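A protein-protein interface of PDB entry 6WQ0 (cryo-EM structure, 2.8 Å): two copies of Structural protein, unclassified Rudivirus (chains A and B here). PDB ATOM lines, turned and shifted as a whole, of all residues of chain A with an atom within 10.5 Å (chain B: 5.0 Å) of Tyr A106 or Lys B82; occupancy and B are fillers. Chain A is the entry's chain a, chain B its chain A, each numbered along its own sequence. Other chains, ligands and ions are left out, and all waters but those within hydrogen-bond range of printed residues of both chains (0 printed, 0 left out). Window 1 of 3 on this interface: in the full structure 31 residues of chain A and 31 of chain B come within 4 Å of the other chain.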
ATOM      1  N   ILE A  75      20.850  19.891   9.409  1.00  0.00           N
ATOM      2  CA  ILE A  75      19.611  20.195  10.122  1.00  0.00           C
ATOM      3  C   ILE A  75      19.915  21.064  11.330  1.00  0.00           C
ATOM      4  O   ILE A  75      19.574  22.252  11.373  1.00  0.00           O
ATOM      5  CB  ILE A  75      18.907  18.896  10.554  1.00  0.00           C
ATOM      6  CG1 ILE A  75      18.598  18.005   9.356  1.00  0.00           C
ATOM      7  CG2 ILE A  75      17.646  19.193  11.350  1.00  0.00           C
ATOM      8  CD1 ILE A  75      18.089  16.648   9.748  1.00  0.00           C
ATOM      9  N   GLY A  78      21.591  24.372  10.570  1.00  0.00           N
ATOM     10  CA  GLY A  78      20.611  25.339  10.123  1.00  0.00           C
ATOM     11  C   GLY A  78      19.806  25.890  11.279  1.00  0.00           C
ATOM     12  O   GLY A  78      19.685  27.108  11.436  1.00  0.00           O
ATOM     13  N   TYR A  79      19.302  25.000  12.139  1.00  0.00           N
ATOM     14  CA  TYR A  79      18.550  25.449  13.301  1.00  0.00           C
ATOM     15  C   TYR A  79      19.355  26.468  14.087  1.00  0.00           C
ATOM     16  O   TYR A  79      18.880  27.577  14.356  1.00  0.00           O
ATOM     17  CB  TYR A  79      18.181  24.256  14.179  1.00  0.00           C
ATOM     18  CG  TYR A  79      17.585  24.639  15.509  1.00  0.00           C
ATOM     19  CD1 TYR A  79      16.225  24.866  15.636  1.00  0.00           C
ATOM     20  CD2 TYR A  79      18.379  24.772  16.640  1.00  0.00           C
ATOM     21  CE1 TYR A  79      15.678  25.217  16.841  1.00  0.00           C
ATOM     22  CE2 TYR A  79      17.835  25.129  17.850  1.00  0.00           C
ATOM     23  CZ  TYR A  79      16.483  25.345  17.944  1.00  0.00           C
ATOM     24  OH  TYR A  79      15.930  25.701  19.148  1.00  0.00           O
ATOM     25  N   GLY A  80      20.610  26.132  14.396  1.00  0.00           N
ATOM     26  CA  GLY A  80      21.428  27.041  15.167  1.00  0.00           C
ATOM     27  C   GLY A  80      21.496  28.407  14.529  1.00  0.00           C
ATOM     28  O   GLY A  80      21.237  29.422  15.182  1.00  0.00           O
ATOM     29  N   LEU A  81      21.755  28.446  13.223  1.00  0.00           N
ATOM     30  CA  LEU A  81      21.881  29.736  12.566  1.00  0.00           C
ATOM     31  C   LEU A  81      20.589  30.520  12.679  1.00  0.00           C
ATOM     32  O   LEU A  81      20.616  31.710  13.011  1.00  0.00           O
ATOM     33  CB  LEU A  81      22.289  29.538  11.110  1.00  0.00           C
ATOM     34  CG  LEU A  81      23.730  29.079  10.897  1.00  0.00           C
ATOM     35  CD1 LEU A  81      23.961  28.735   9.446  1.00  0.00           C
ATOM     36  CD2 LEU A  81      24.702  30.143  11.353  1.00  0.00           C
ATOM     37  N   LYS A  82      19.452  29.847  12.493  1.00  0.00           N
ATOM     38  CA  LYS A  82      18.166  30.508  12.648  1.00  0.00           C
ATOM     39  C   LYS A  82      18.059  31.176  14.010  1.00  0.00           C
ATOM     40  O   LYS A  82      17.721  32.362  14.102  1.00  0.00           O
ATOM     41  CB  LYS A  82      17.044  29.495  12.446  1.00  0.00           C
ATOM     42  CG  LYS A  82      15.720  30.086  12.064  1.00  0.00           C
ATOM     43  CD  LYS A  82      15.641  30.345  10.598  1.00  0.00           C
ATOM     44  CE  LYS A  82      14.240  30.690  10.164  1.00  0.00           C
ATOM     45  NZ  LYS A  82      13.353  29.527  10.356  1.00  0.00           N
ATOM     46  N   VAL A  83      18.395  30.447  15.078  1.00  0.00           N
ATOM     47  CA  VAL A  83      18.333  31.034  16.412  1.00  0.00           C
ATOM     48  C   VAL A  83      19.229  32.258  16.482  1.00  0.00           C
ATOM     49  O   VAL A  83      18.803  33.331  16.928  1.00  0.00           O
ATOM     50  CB  VAL A  83      18.707  29.988  17.476  1.00  0.00           C
ATOM     51  CG1 VAL A  83      18.791  30.630  18.841  1.00  0.00           C
ATOM     52  CG2 VAL A  83      17.697  28.873  17.489  1.00  0.00           C
ATOM     53  N   ARG A  85      20.092  34.164  14.096  1.00  0.00           N
ATOM     54  CA  ARG A  85      19.419  35.222  13.355  1.00  0.00           C
ATOM     55  C   ARG A  85      18.470  35.985  14.260  1.00  0.00           C
ATOM     56  O   ARG A  85      18.546  37.214  14.363  1.00  0.00           O
ATOM     57  CB  ARG A  85      18.672  34.638  12.159  1.00  0.00           C
ATOM     58  CG  ARG A  85      17.843  35.645  11.403  1.00  0.00           C
ATOM     59  CD  ARG A  85      17.444  35.121  10.051  1.00  0.00           C
ATOM     60  NE  ARG A  85      16.457  35.975   9.399  1.00  0.00           N
ATOM     61  CZ  ARG A  85      15.221  35.599   9.099  1.00  0.00           C
ATOM     62  NH1 ARG A  85      14.816  34.374   9.378  1.00  0.00           N
ATOM     63  NH2 ARG A  85      14.392  36.442   8.508  1.00  0.00           N
ATOM     64  N   ASN A  98       9.662  33.250  22.503  1.00  0.00           N
ATOM     65  CA  ASN A  98       8.598  32.821  21.599  1.00  0.00           C
ATOM     66  C   ASN A  98       9.174  32.297  20.291  1.00  0.00           C
ATOM     67  O   ASN A  98       8.708  31.286  19.751  1.00  0.00           O
ATOM     68  CB  ASN A  98       7.638  33.976  21.331  1.00  0.00           C
ATOM     69  CG  ASN A  98       6.911  34.425  22.571  1.00  0.00           C
ATOM     70  OD1 ASN A  98       6.881  33.721  23.576  1.00  0.00           O
ATOM     71  ND2 ASN A  98       6.320  35.606  22.512  1.00  0.00           N
ATOM     72  N   MET A  99      10.201  32.966  19.774  1.00  0.00           N
ATOM     73  CA  MET A  99      10.775  32.519  18.512  1.00  0.00           C
ATOM     74  C   MET A  99      11.546  31.215  18.659  1.00  0.00           C
ATOM     75  O   MET A  99      11.522  30.392  17.743  1.00  0.00           O
ATOM     76  CB  MET A  99      11.656  33.604  17.907  1.00  0.00           C
ATOM     77  CG  MET A  99      10.843  34.728  17.306  1.00  0.00           C
ATOM     78  SD  MET A  99      11.761  35.680  16.101  1.00  0.00           S
ATOM     79  CE  MET A  99      11.756  34.526  14.735  1.00  0.00           C
ATOM     80  N   VAL A 100      12.209  30.987  19.796  1.00  0.00           N
ATOM     81  CA  VAL A 100      12.864  29.699  20.017  1.00  0.00           C
ATOM     82  C   VAL A 100      11.838  28.577  20.084  1.00  0.00           C
ATOM     83  O   VAL A 100      12.040  27.501  19.508  1.00  0.00           O
ATOM     84  CB  VAL A 100      13.743  29.742  21.281  1.00  0.00           C
ATOM     85  CG1 VAL A 100      14.308  28.369  21.582  1.00  0.00           C
ATOM     86  CG2 VAL A 100      14.885  30.702  21.077  1.00  0.00           C
ATOM     87  N   ALA A 101      10.717  28.806  20.771  1.00  0.00           N
ATOM     88  CA  ALA A 101       9.679  27.779  20.828  1.00  0.00           C
ATOM     89  C   ALA A 101       9.107  27.490  19.444  1.00  0.00           C
ATOM     90  O   ALA A 101       8.927  26.323  19.063  1.00  0.00           O
ATOM     91  CB  ALA A 101       8.573  28.205  21.789  1.00  0.00           C
ATOM     92  N   GLY A 102       8.826  28.540  18.671  1.00  0.00           N
ATOM     93  CA  GLY A 102       8.297  28.342  17.332  1.00  0.00           C
ATOM     94  C   GLY A 102       9.270  27.646  16.402  1.00  0.00           C
ATOM     95  O   GLY A 102       8.871  26.808  15.592  1.00  0.00           O
ATOM     96  N   LEU A 103      10.559  27.973  16.508  1.00  0.00           N
ATOM     97  CA  LEU A 103      11.565  27.316  15.679  1.00  0.00           C
ATOM     98  C   LEU A 103      11.727  25.855  16.060  1.00  0.00           C
ATOM     99  O   LEU A 103      11.927  25.000  15.190  1.00  0.00           O
ATOM    100  CB  LEU A 103      12.898  28.046  15.798  1.00  0.00           C
ATOM    101  CG  LEU A 103      12.962  29.406  15.122  1.00  0.00           C
ATOM    102  CD1 LEU A 103      14.314  30.039  15.354  1.00  0.00           C
ATOM    103  CD2 LEU A 103      12.668  29.266  13.648  1.00  0.00           C
ATOM    104  N   LYS A 104      11.652  25.544  17.353  1.00  0.00           N
ATOM    105  CA  LYS A 104      11.726  24.150  17.763  1.00  0.00           C
ATOM    106  C   LYS A 104      10.546  23.359  17.223  1.00  0.00           C
ATOM    107  O   LYS A 104      10.723  22.249  16.713  1.00  0.00           O
ATOM    108  CB  LYS A 104      11.803  24.050  19.284  1.00  0.00           C
ATOM    109  CG  LYS A 104      13.213  23.888  19.794  1.00  0.00           C
ATOM    110  CD  LYS A 104      13.241  23.554  21.263  1.00  0.00           C
ATOM    111  CE  LYS A 104      14.413  24.227  21.942  1.00  0.00           C
ATOM    112  NZ  LYS A 104      14.258  24.231  23.414  1.00  0.00           N
ATOM    113  N   ALA A 105       9.334  23.909  17.320  1.00  0.00           N
ATOM    114  CA  ALA A 105       8.175  23.222  16.751  1.00  0.00           C
ATOM    115  C   ALA A 105       8.339  23.029  15.248  1.00  0.00           C
ATOM    116  O   ALA A 105       8.122  21.928  14.720  1.00  0.00           O
ATOM    117  CB  ALA A 105       6.899  24.002  17.057  1.00  0.00           C
ATOM    118  N   TYR A 106       8.726  24.096  14.545  1.00  0.00           N
ATOM    119  CA  TYR A 106       9.013  24.021  13.118  1.00  0.00           C
ATOM    120  C   TYR A 106       9.925  22.847  12.797  1.00  0.00           C
ATOM    121  O   TYR A 106       9.559  21.959  12.024  1.00  0.00           O
ATOM    122  CB  TYR A 106       9.646  25.340  12.673  1.00  0.00           C
ATOM    123  CG  TYR A 106      10.066  25.431  11.225  1.00  0.00           C
ATOM    124  CD1 TYR A 106       9.411  24.717  10.236  1.00  0.00           C
ATOM    125  CD2 TYR A 106      11.110  26.259  10.851  1.00  0.00           C
ATOM    126  CE1 TYR A 106       9.795  24.817   8.922  1.00  0.00           C
ATOM    127  CE2 TYR A 106      11.501  26.360   9.543  1.00  0.00           C
ATOM    128  CZ  TYR A 106      10.843  25.638   8.582  1.00  0.00           C
ATOM    129  OH  TYR A 106      11.235  25.740   7.272  1.00  0.00           O
ATOM    130  N   TYR A 107      11.116  22.822  13.397  1.00  0.00           N
ATOM    131  CA  TYR A 107      12.106  21.814  13.033  1.00  0.00           C
ATOM    132  C   TYR A 107      11.677  20.412  13.442  1.00  0.00           C
ATOM    133  O   TYR A 107      11.783  19.482  12.638  1.00  0.00           O
ATOM    134  CB  TYR A 107      13.460  22.165  13.642  1.00  0.00           C
ATOM    135  CG  TYR A 107      14.355  22.882  12.671  1.00  0.00           C
ATOM    136  CD1 TYR A 107      15.417  22.232  12.075  1.00  0.00           C
ATOM    137  CD2 TYR A 107      14.122  24.202  12.330  1.00  0.00           C
ATOM    138  CE1 TYR A 107      16.224  22.877  11.175  1.00  0.00           C
ATOM    139  CE2 TYR A 107      14.926  24.856  11.434  1.00  0.00           C
ATOM    140  CZ  TYR A 107      15.976  24.189  10.860  1.00  0.00           C
ATOM    141  OH  TYR A 107      16.785  24.834   9.963  1.00  0.00           O
ATOM    142  N   VAL A 108      11.165  20.243  14.659  1.00  0.00           N
ATOM    143  CA  VAL A 108      10.771  18.919  15.122  1.00  0.00           C
ATOM    144  C   VAL A 108       9.678  18.327  14.246  1.00  0.00           C
ATOM    145  O   VAL A 108       9.739  17.149  13.879  1.00  0.00           O
ATOM    146  CB  VAL A 108      10.339  18.984  16.597  1.00  0.00           C
ATOM    147  CG1 VAL A 108       9.760  17.665  17.027  1.00  0.00           C
ATOM    148  CG2 VAL A 108      11.517  19.317  17.473  1.00  0.00           C
ATOM    149  N   SER A 109       8.664  19.116  13.886  1.00  0.00           N
ATOM    150  CA  SER A 109       7.520  18.512  13.214  1.00  0.00           C
ATOM    151  C   SER A 109       7.662  18.527  11.697  1.00  0.00           C
ATOM    152  O   SER A 109       7.004  17.739  11.011  1.00  0.00           O
ATOM    153  CB  SER A 109       6.229  19.205  13.644  1.00  0.00           C
ATOM    154  OG  SER A 109       6.223  20.559  13.250  1.00  0.00           O
ATOM    155  N   ALA A 110       8.500  19.403  11.144  1.00  0.00           N
ATOM    156  CA  ALA A 110       8.667  19.426   9.700  1.00  0.00           C
ATOM    157  C   ALA A 110       9.834  18.570   9.234  1.00  0.00           C
ATOM    158  O   ALA A 110       9.742  17.932   8.182  1.00  0.00           O
ATOM    159  CB  ALA A 110       8.852  20.864   9.213  1.00  0.00           C
ATOM    160  N   TYR A 111      10.934  18.531   9.988  1.00  0.00           N
ATOM    161  CA  TYR A 111      12.149  17.869   9.536  1.00  0.00           C
ATOM    162  C   TYR A 111      12.561  16.706  10.426  1.00  0.00           C
ATOM    163  O   TYR A 111      13.638  16.139  10.222  1.00  0.00           O
ATOM    164  CB  TYR A 111      13.282  18.889   9.434  1.00  0.00           C
ATOM    165  CG  TYR A 111      12.949  20.020   8.499  1.00  0.00           C
ATOM    166  CD1 TYR A 111      12.484  19.767   7.221  1.00  0.00           C
ATOM    167  CD2 TYR A 111      13.068  21.338   8.900  1.00  0.00           C
ATOM    168  CE1 TYR A 111      12.166  20.786   6.368  1.00  0.00           C
ATOM    169  CE2 TYR A 111      12.754  22.368   8.049  1.00  0.00           C
ATOM    170  CZ  TYR A 111      12.301  22.082   6.783  1.00  0.00           C
ATOM    171  OH  TYR A 111      11.981  23.099   5.920  1.00  0.00           O
ATOM    172  N   GLY A 112      11.735  16.329  11.397  1.00  0.00           N
ATOM    173  CA  GLY A 112      12.030  15.171  12.220  1.00  0.00           C
ATOM    174  C   GLY A 112      13.289  15.295  13.044  1.00  0.00           C
ATOM    175  O   GLY A 112      13.959  14.289  13.293  1.00  0.00           O
ATOM    176  N   ALA A 113      13.629  16.503  13.480  1.00  0.00           N
ATOM    177  CA  ALA A 113      14.810  16.713  14.295  1.00  0.00           C
ATOM    178  C   ALA A 113      14.594  16.168  15.701  1.00  0.00           C
ATOM    179  O   ALA A 113      13.467  16.018  16.173  1.00  0.00           O
ATOM    180  CB  ALA A 113      15.166  18.196  14.352  1.00  0.00           C
ATOM    181  N   ASN A 114      15.702  15.866  16.366  1.00  0.00           N
ATOM    182  CA  ASN A 114      15.733  15.312  17.716  1.00  0.00           C
ATOM    183  C   ASN A 114      15.567  16.429  18.738  1.00  0.00           C
ATOM    184  O   ASN A 114      16.320  17.408  18.700  1.00  0.00           O
ATOM    185  CB  ASN A 114      17.046  14.584  17.959  1.00  0.00           C
ATOM    186  CG  ASN A 114      16.967  13.585  19.093  1.00  0.00           C
ATOM    187  OD1 ASN A 114      16.043  13.601  19.898  1.00  0.00           O
ATOM    188  ND2 ASN A 114      17.955  12.706  19.161  1.00  0.00           N
ATOM    189  N   LEU A 118      18.341  19.508  19.729  1.00  0.00           N
ATOM    190  CA  LEU A 118      17.892  20.891  19.612  1.00  0.00           C
ATOM    191  C   LEU A 118      18.070  21.632  20.929  1.00  0.00           C
ATOM    192  O   LEU A 118      18.460  22.806  20.943  1.00  0.00           O
ATOM    193  CB  LEU A 118      16.436  20.939  19.156  1.00  0.00           C
ATOM    194  CG  LEU A 118      16.177  20.636  17.682  1.00  0.00           C
ATOM    195  CD1 LEU A 118      14.734  20.878  17.342  1.00  0.00           C
ATOM    196  CD2 LEU A 118      17.070  21.477  16.801  1.00  0.00           C
ATOM    197  N   GLN B  77       0.225  35.838   3.986  1.00  0.00           N
ATOM    198  CA  GLN B  77       0.879  35.830   2.686  1.00  0.00           C
ATOM    199  C   GLN B  77       2.167  35.032   2.751  1.00  0.00           C
ATOM    200  O   GLN B  77       2.355  34.081   1.980  1.00  0.00           O
ATOM    201  CB  GLN B  77       1.149  37.256   2.214  1.00  0.00           C
ATOM    202  CG  GLN B  77      -0.076  37.977   1.689  1.00  0.00           C
ATOM    203  CD  GLN B  77      -0.518  37.480   0.332  1.00  0.00           C
ATOM    204  OE1 GLN B  77       0.166  36.692  -0.306  1.00  0.00           O
ATOM    205  NE2 GLN B  77      -1.668  37.944  -0.117  1.00  0.00           N
ATOM    206  N   GLY B  78       3.022  35.344   3.727  1.00  0.00           N
ATOM    207  CA  GLY B  78       4.249  34.592   3.879  1.00  0.00           C
ATOM    208  C   GLY B  78       3.980  33.111   4.013  1.00  0.00           C
ATOM    209  O   GLY B  78       4.528  32.305   3.255  1.00  0.00           O
ATOM    210  N   TYR B  79       3.065  32.742   4.914  1.00  0.00           N
ATOM    211  CA  TYR B  79       2.734  31.334   5.076  1.00  0.00           C
ATOM    212  C   TYR B  79       2.344  30.731   3.740  1.00  0.00           C
ATOM    213  O   TYR B  79       2.921  29.726   3.307  1.00  0.00           O
ATOM    214  CB  TYR B  79       1.610  31.162   6.095  1.00  0.00           C
ATOM    215  CG  TYR B  79       1.080  29.751   6.184  1.00  0.00           C
ATOM    216  CD1 TYR B  79       1.741  28.788   6.930  1.00  0.00           C
ATOM    217  CD2 TYR B  79      -0.081  29.378   5.522  1.00  0.00           C
ATOM    218  CE1 TYR B  79       1.263  27.505   7.010  1.00  0.00           C
ATOM    219  CE2 TYR B  79      -0.561  28.097   5.598  1.00  0.00           C
ATOM    220  CZ  TYR B  79       0.112  27.165   6.344  1.00  0.00           C
ATOM    221  OH  TYR B  79      -0.374  25.886   6.416  1.00  0.00           O
ATOM    222  N   GLY B  80       1.424  31.390   3.031  1.00  0.00           N
ATOM    223  CA  GLY B  80       1.004  30.877   1.744  1.00  0.00           C
ATOM    224  C   GLY B  80       2.182  30.620   0.833  1.00  0.00           C
ATOM    225  O   GLY B  80       2.356  29.507   0.331  1.00  0.00           O
ATOM    226  N   LEU B  81       3.052  31.619   0.676  1.00  0.00           N
ATOM    227  CA  LEU B  81       4.177  31.442  -0.227  1.00  0.00           C
ATOM    228  C   LEU B  81       5.055  30.299   0.240  1.00  0.00           C
ATOM    229  O   LEU B  81       5.430  29.438  -0.562  1.00  0.00           O
ATOM    230  CB  LEU B  81       4.975  32.736  -0.339  1.00  0.00           C
ATOM    231  CG  LEU B  81       4.245  33.938  -0.936  1.00  0.00           C
ATOM    232  CD1 LEU B  81       5.129  35.160  -0.878  1.00  0.00           C
ATOM    233  CD2 LEU B  81       3.817  33.654  -2.355  1.00  0.00           C
ATOM    234  N   LYS B  82       5.306  30.230   1.549  1.00  0.00           N
ATOM    235  CA  LYS B  82       6.062  29.120   2.109  1.00  0.00           C
ATOM    236  C   LYS B  82       5.470  27.792   1.667  1.00  0.00           C
ATOM    237  O   LYS B  82       6.179  26.945   1.110  1.00  0.00           O
ATOM    238  CB  LYS B  82       6.082  29.237   3.631  1.00  0.00           C
ATOM    239  CG  LYS B  82       7.127  28.409   4.324  1.00  0.00           C
ATOM    240  CD  LYS B  82       8.501  28.978   4.153  1.00  0.00           C
ATOM    241  CE  LYS B  82       9.516  28.239   4.991  1.00  0.00           C
ATOM    242  NZ  LYS B  82       9.249  28.462   6.426  1.00  0.00           N
ATOM    243  N   VAL B  83       4.158  27.621   1.835  1.00  0.00           N
ATOM    244  CA  VAL B  83       3.524  26.366   1.444  1.00  0.00           C
ATOM    245  C   VAL B  83       3.754  26.096  -0.033  1.00  0.00           C
ATOM    246  O   VAL B  83       4.154  24.993  -0.419  1.00  0.00           O
ATOM    247  CB  VAL B  83       2.025  26.393   1.787  1.00  0.00           C
ATOM    248  CG1 VAL B  83       1.338  25.188   1.197  1.00  0.00           C
ATOM    249  CG2 VAL B  83       1.828  26.429   3.283  1.00  0.00           C
ATOM    250  N   ALA B  84       3.548  27.112  -0.876  1.00  0.00           N
ATOM    251  CA  ALA B  84       3.753  26.919  -2.304  1.00  0.00           C
ATOM    252  C   ALA B  84       5.174  26.473  -2.591  1.00  0.00           C
ATOM    253  O   ALA B  84       5.390  25.577  -3.415  1.00  0.00           O
ATOM    254  CB  ALA B  84       3.423  28.203  -3.060  1.00  0.00           C
ATOM    255  N   ARG B  85       6.146  27.041  -1.873  1.00  0.00           N
ATOM    256  CA  ARG B  85       7.530  26.613  -2.023  1.00  0.00           C
ATOM    257  C   ARG B  85       7.639  25.104  -1.878  1.00  0.00           C
ATOM    258  O   ARG B  85       8.151  24.419  -2.771  1.00  0.00           O
ATOM    259  CB  ARG B  85       8.402  27.332  -0.997  1.00  0.00           C
ATOM    260  CG  ARG B  85       9.880  27.081  -1.140  1.00  0.00           C
ATOM    261  CD  ARG B  85      10.657  27.866  -0.120  1.00  0.00           C
ATOM    262  NE  ARG B  85      12.050  27.448  -0.031  1.00  0.00           N
ATOM    263  CZ  ARG B  85      12.599  26.916   1.053  1.00  0.00           C
ATOM    264  NH1 ARG B  85      11.873  26.737   2.143  1.00  0.00           N
ATOM    265  NH2 ARG B  85      13.875  26.562   1.047  1.00  0.00           N
ATOM    266  N   ALA B  86       7.084  24.560  -0.792  1.00  0.00           N
ATOM    267  CA  ALA B  86       7.133  23.120  -0.582  1.00  0.00           C
ATOM    268  C   ALA B  86       6.530  22.377  -1.763  1.00  0.00           C
ATOM    269  O   ALA B  86       7.140  21.441  -2.293  1.00  0.00           O
ATOM    270  CB  ALA B  86       6.414  22.753   0.712  1.00  0.00           C
ATOM    271  N   GLY B 102       4.360  21.040   9.868  1.00  0.00           N
ATOM    272  CA  GLY B 102       5.470  21.744  10.490  1.00  0.00           C
ATOM    273  C   GLY B 102       5.410  23.247  10.297  1.00  0.00           C
ATOM    274  O   GLY B 102       5.759  24.011  11.198  1.00  0.00           O
ATOM    275  N   LEU B 103       4.954  23.692   9.127  1.00  0.00           N
ATOM    276  CA  LEU B 103       4.823  25.122   8.874  1.00  0.00           C
ATOM    277  C   LEU B 103       3.719  25.738   9.718  1.00  0.00           C
ATOM    278  O   LEU B 103       3.866  26.862  10.215  1.00  0.00           O
ATOM    279  CB  LEU B 103       4.556  25.361   7.394  1.00  0.00           C
ATOM    280  CG  LEU B 103       5.759  25.166   6.482  1.00  0.00           C
ATOM    281  CD1 LEU B 103       5.371  25.419   5.043  1.00  0.00           C
ATOM    282  CD2 LEU B 103       6.883  26.074   6.918  1.00  0.00           C
ATOM    283  N   ALA B 105       2.750  24.623  12.681  1.00  0.00           N
ATOM    284  CA  ALA B 105       3.342  24.711  14.015  1.00  0.00           C
ATOM    285  C   ALA B 105       4.258  25.922  14.126  1.00  0.00           C
ATOM    286  O   ALA B 105       4.170  26.700  15.083  1.00  0.00           O
ATOM    287  CB  ALA B 105       4.107  23.430  14.335  1.00  0.00           C
ATOM    288  N   TYR B 106       5.138  26.097  13.137  1.00  0.00           N
ATOM    289  CA  TYR B 106       6.052  27.235  13.104  1.00  0.00           C
ATOM    290  C   TYR B 106       5.308  28.553  13.256  1.00  0.00           C
ATOM    291  O   TYR B 106       5.620  29.355  14.142  1.00  0.00           O
ATOM    292  CB  TYR B 106       6.830  27.202  11.788  1.00  0.00           C
ATOM    293  CG  TYR B 106       7.793  28.341  11.544  1.00  0.00           C
ATOM    294  CD1 TYR B 106       8.467  28.952  12.588  1.00  0.00           C
ATOM    295  CD2 TYR B 106       8.050  28.778  10.257  1.00  0.00           C
ATOM    296  CE1 TYR B 106       9.349  29.979  12.354  1.00  0.00           C
ATOM    297  CE2 TYR B 106       8.931  29.802  10.014  1.00  0.00           C
ATOM    298  CZ  TYR B 106       9.577  30.399  11.063  1.00  0.00           C
ATOM    299  OH  TYR B 106      10.456  31.423  10.817  1.00  0.00           O
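The side-chain amino group (NZ) of Lys B82 sits at hydrogen-bond distance from the side-chain hydroxyl (OH) of Tyr A106 (3.5 Å). OH of Tyr B106 lies within hydrogen-bond range of NZ of Lys A82.
O of Ala A105 lies within hydrogen-bond range of OG of Ser A109 (2.8 Å). OH of Tyr A111 lies within hydrogen-bond range of OH of Tyr A106 (3.1 Å).
Among the printed residues, merely in contact across the chains: Ser A109 with Gly B102, Tyr A106 with Tyr B106, Leu A103 with Tyr B106, Gly A102 with Tyr B106, Ala A110 with Gly B102, Ser A109 with Ala B105, Tyr A106 with Leu B103, Tyr A106 with Gly B102 and Ala A105 with Ala B105.
Printed residues of chain B within 4 Å of Lys A82: Tyr B106. Val A83 touches none of the printed residues of chain B. Printed residues of chain B within 4 Å of Ala A105: Ala B105 (3.9 Å). Tyr A106 touches four residues of chain B. Of the printed residues of chain B, Ser A109 touches Gly B102 (3.1 Å) and Ala B105 (3.7 Å). Of the printed residues of chain B, Ala A110 touches Gly B102. Tyr A111 touches none of the printed residues of chain B. No residue of chain A comes within 4 Å of Gly B78. No residue of chain A comes within 4 Å of Gly B80. No residue of chain A comes within 4 Å of Leu B81. Lys B82 touches just one residue of chain A: Tyr A106 (3.5 Å). Ala B84 touches none of the printed residues of chain A. Leu B103 touches one residue of chain A. Ala B105 touches just these residues of chain A: Ala A105 (3.9 Å) and Ser A109 (3.7 Å). Tyr B106 touches just these residues of chain A: Lys A82, Gly A102, Leu A103 and Tyr A106. The nearest residue of chain B that does not touch Tyr A106 is Ala B105 (4.7 Å). The nearest printed residue of chain A that does not touch Lys B82 is Tyr A111 (5.8 Å). The nearest printed residue of chain B that does not touch Ala A110 is Leu B103 (4.8 Å).
Hydrophobic or aromatic side chains of chain B within 4 Å of the printed part of chain A: Leu B103, Ala B105 and Tyr B106. Of the 26 printed residues of chain A, 7 touch a printed residue of chain B. Printed residues of chain A that touch a printed residue of chain B: Lys A82, Gly A102, Leu A103, Ala A105, Tyr A106, Ser A109 and Ala A110. Hydrophobic or aromatic side chains of chain A within 4 Å of the printed part of chain B: Leu A103, Ala A105, Tyr A106 and Ala A110. Among the printed residues, 11 pairs touch across the chains. Among the printed residues, no Asp or Glu carboxylate lies within 4 Å of a Lys or Arg side-chain nitrogen of the other chain.
Lys A82 touches Tyr B106, and with the chains exchanged Tyr A106 touches Lys B82. Gly A102 touches Tyr B106, and with the chains exchanged Tyr A106 touches Gly B102. Leu A103 touches Tyr B106, and with the chains exchanged Tyr A106 touches Leu B103. Ala A105 touches its own counterpart, Ala B105. Positions printed for both chains: 78, 79, 80, 81, 82, 83, 85, 102, 103, 105 and 106. Of the 11 pairs that touch across the chains among the printed residues, 8 have their exchanged pair printed and touching as well.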
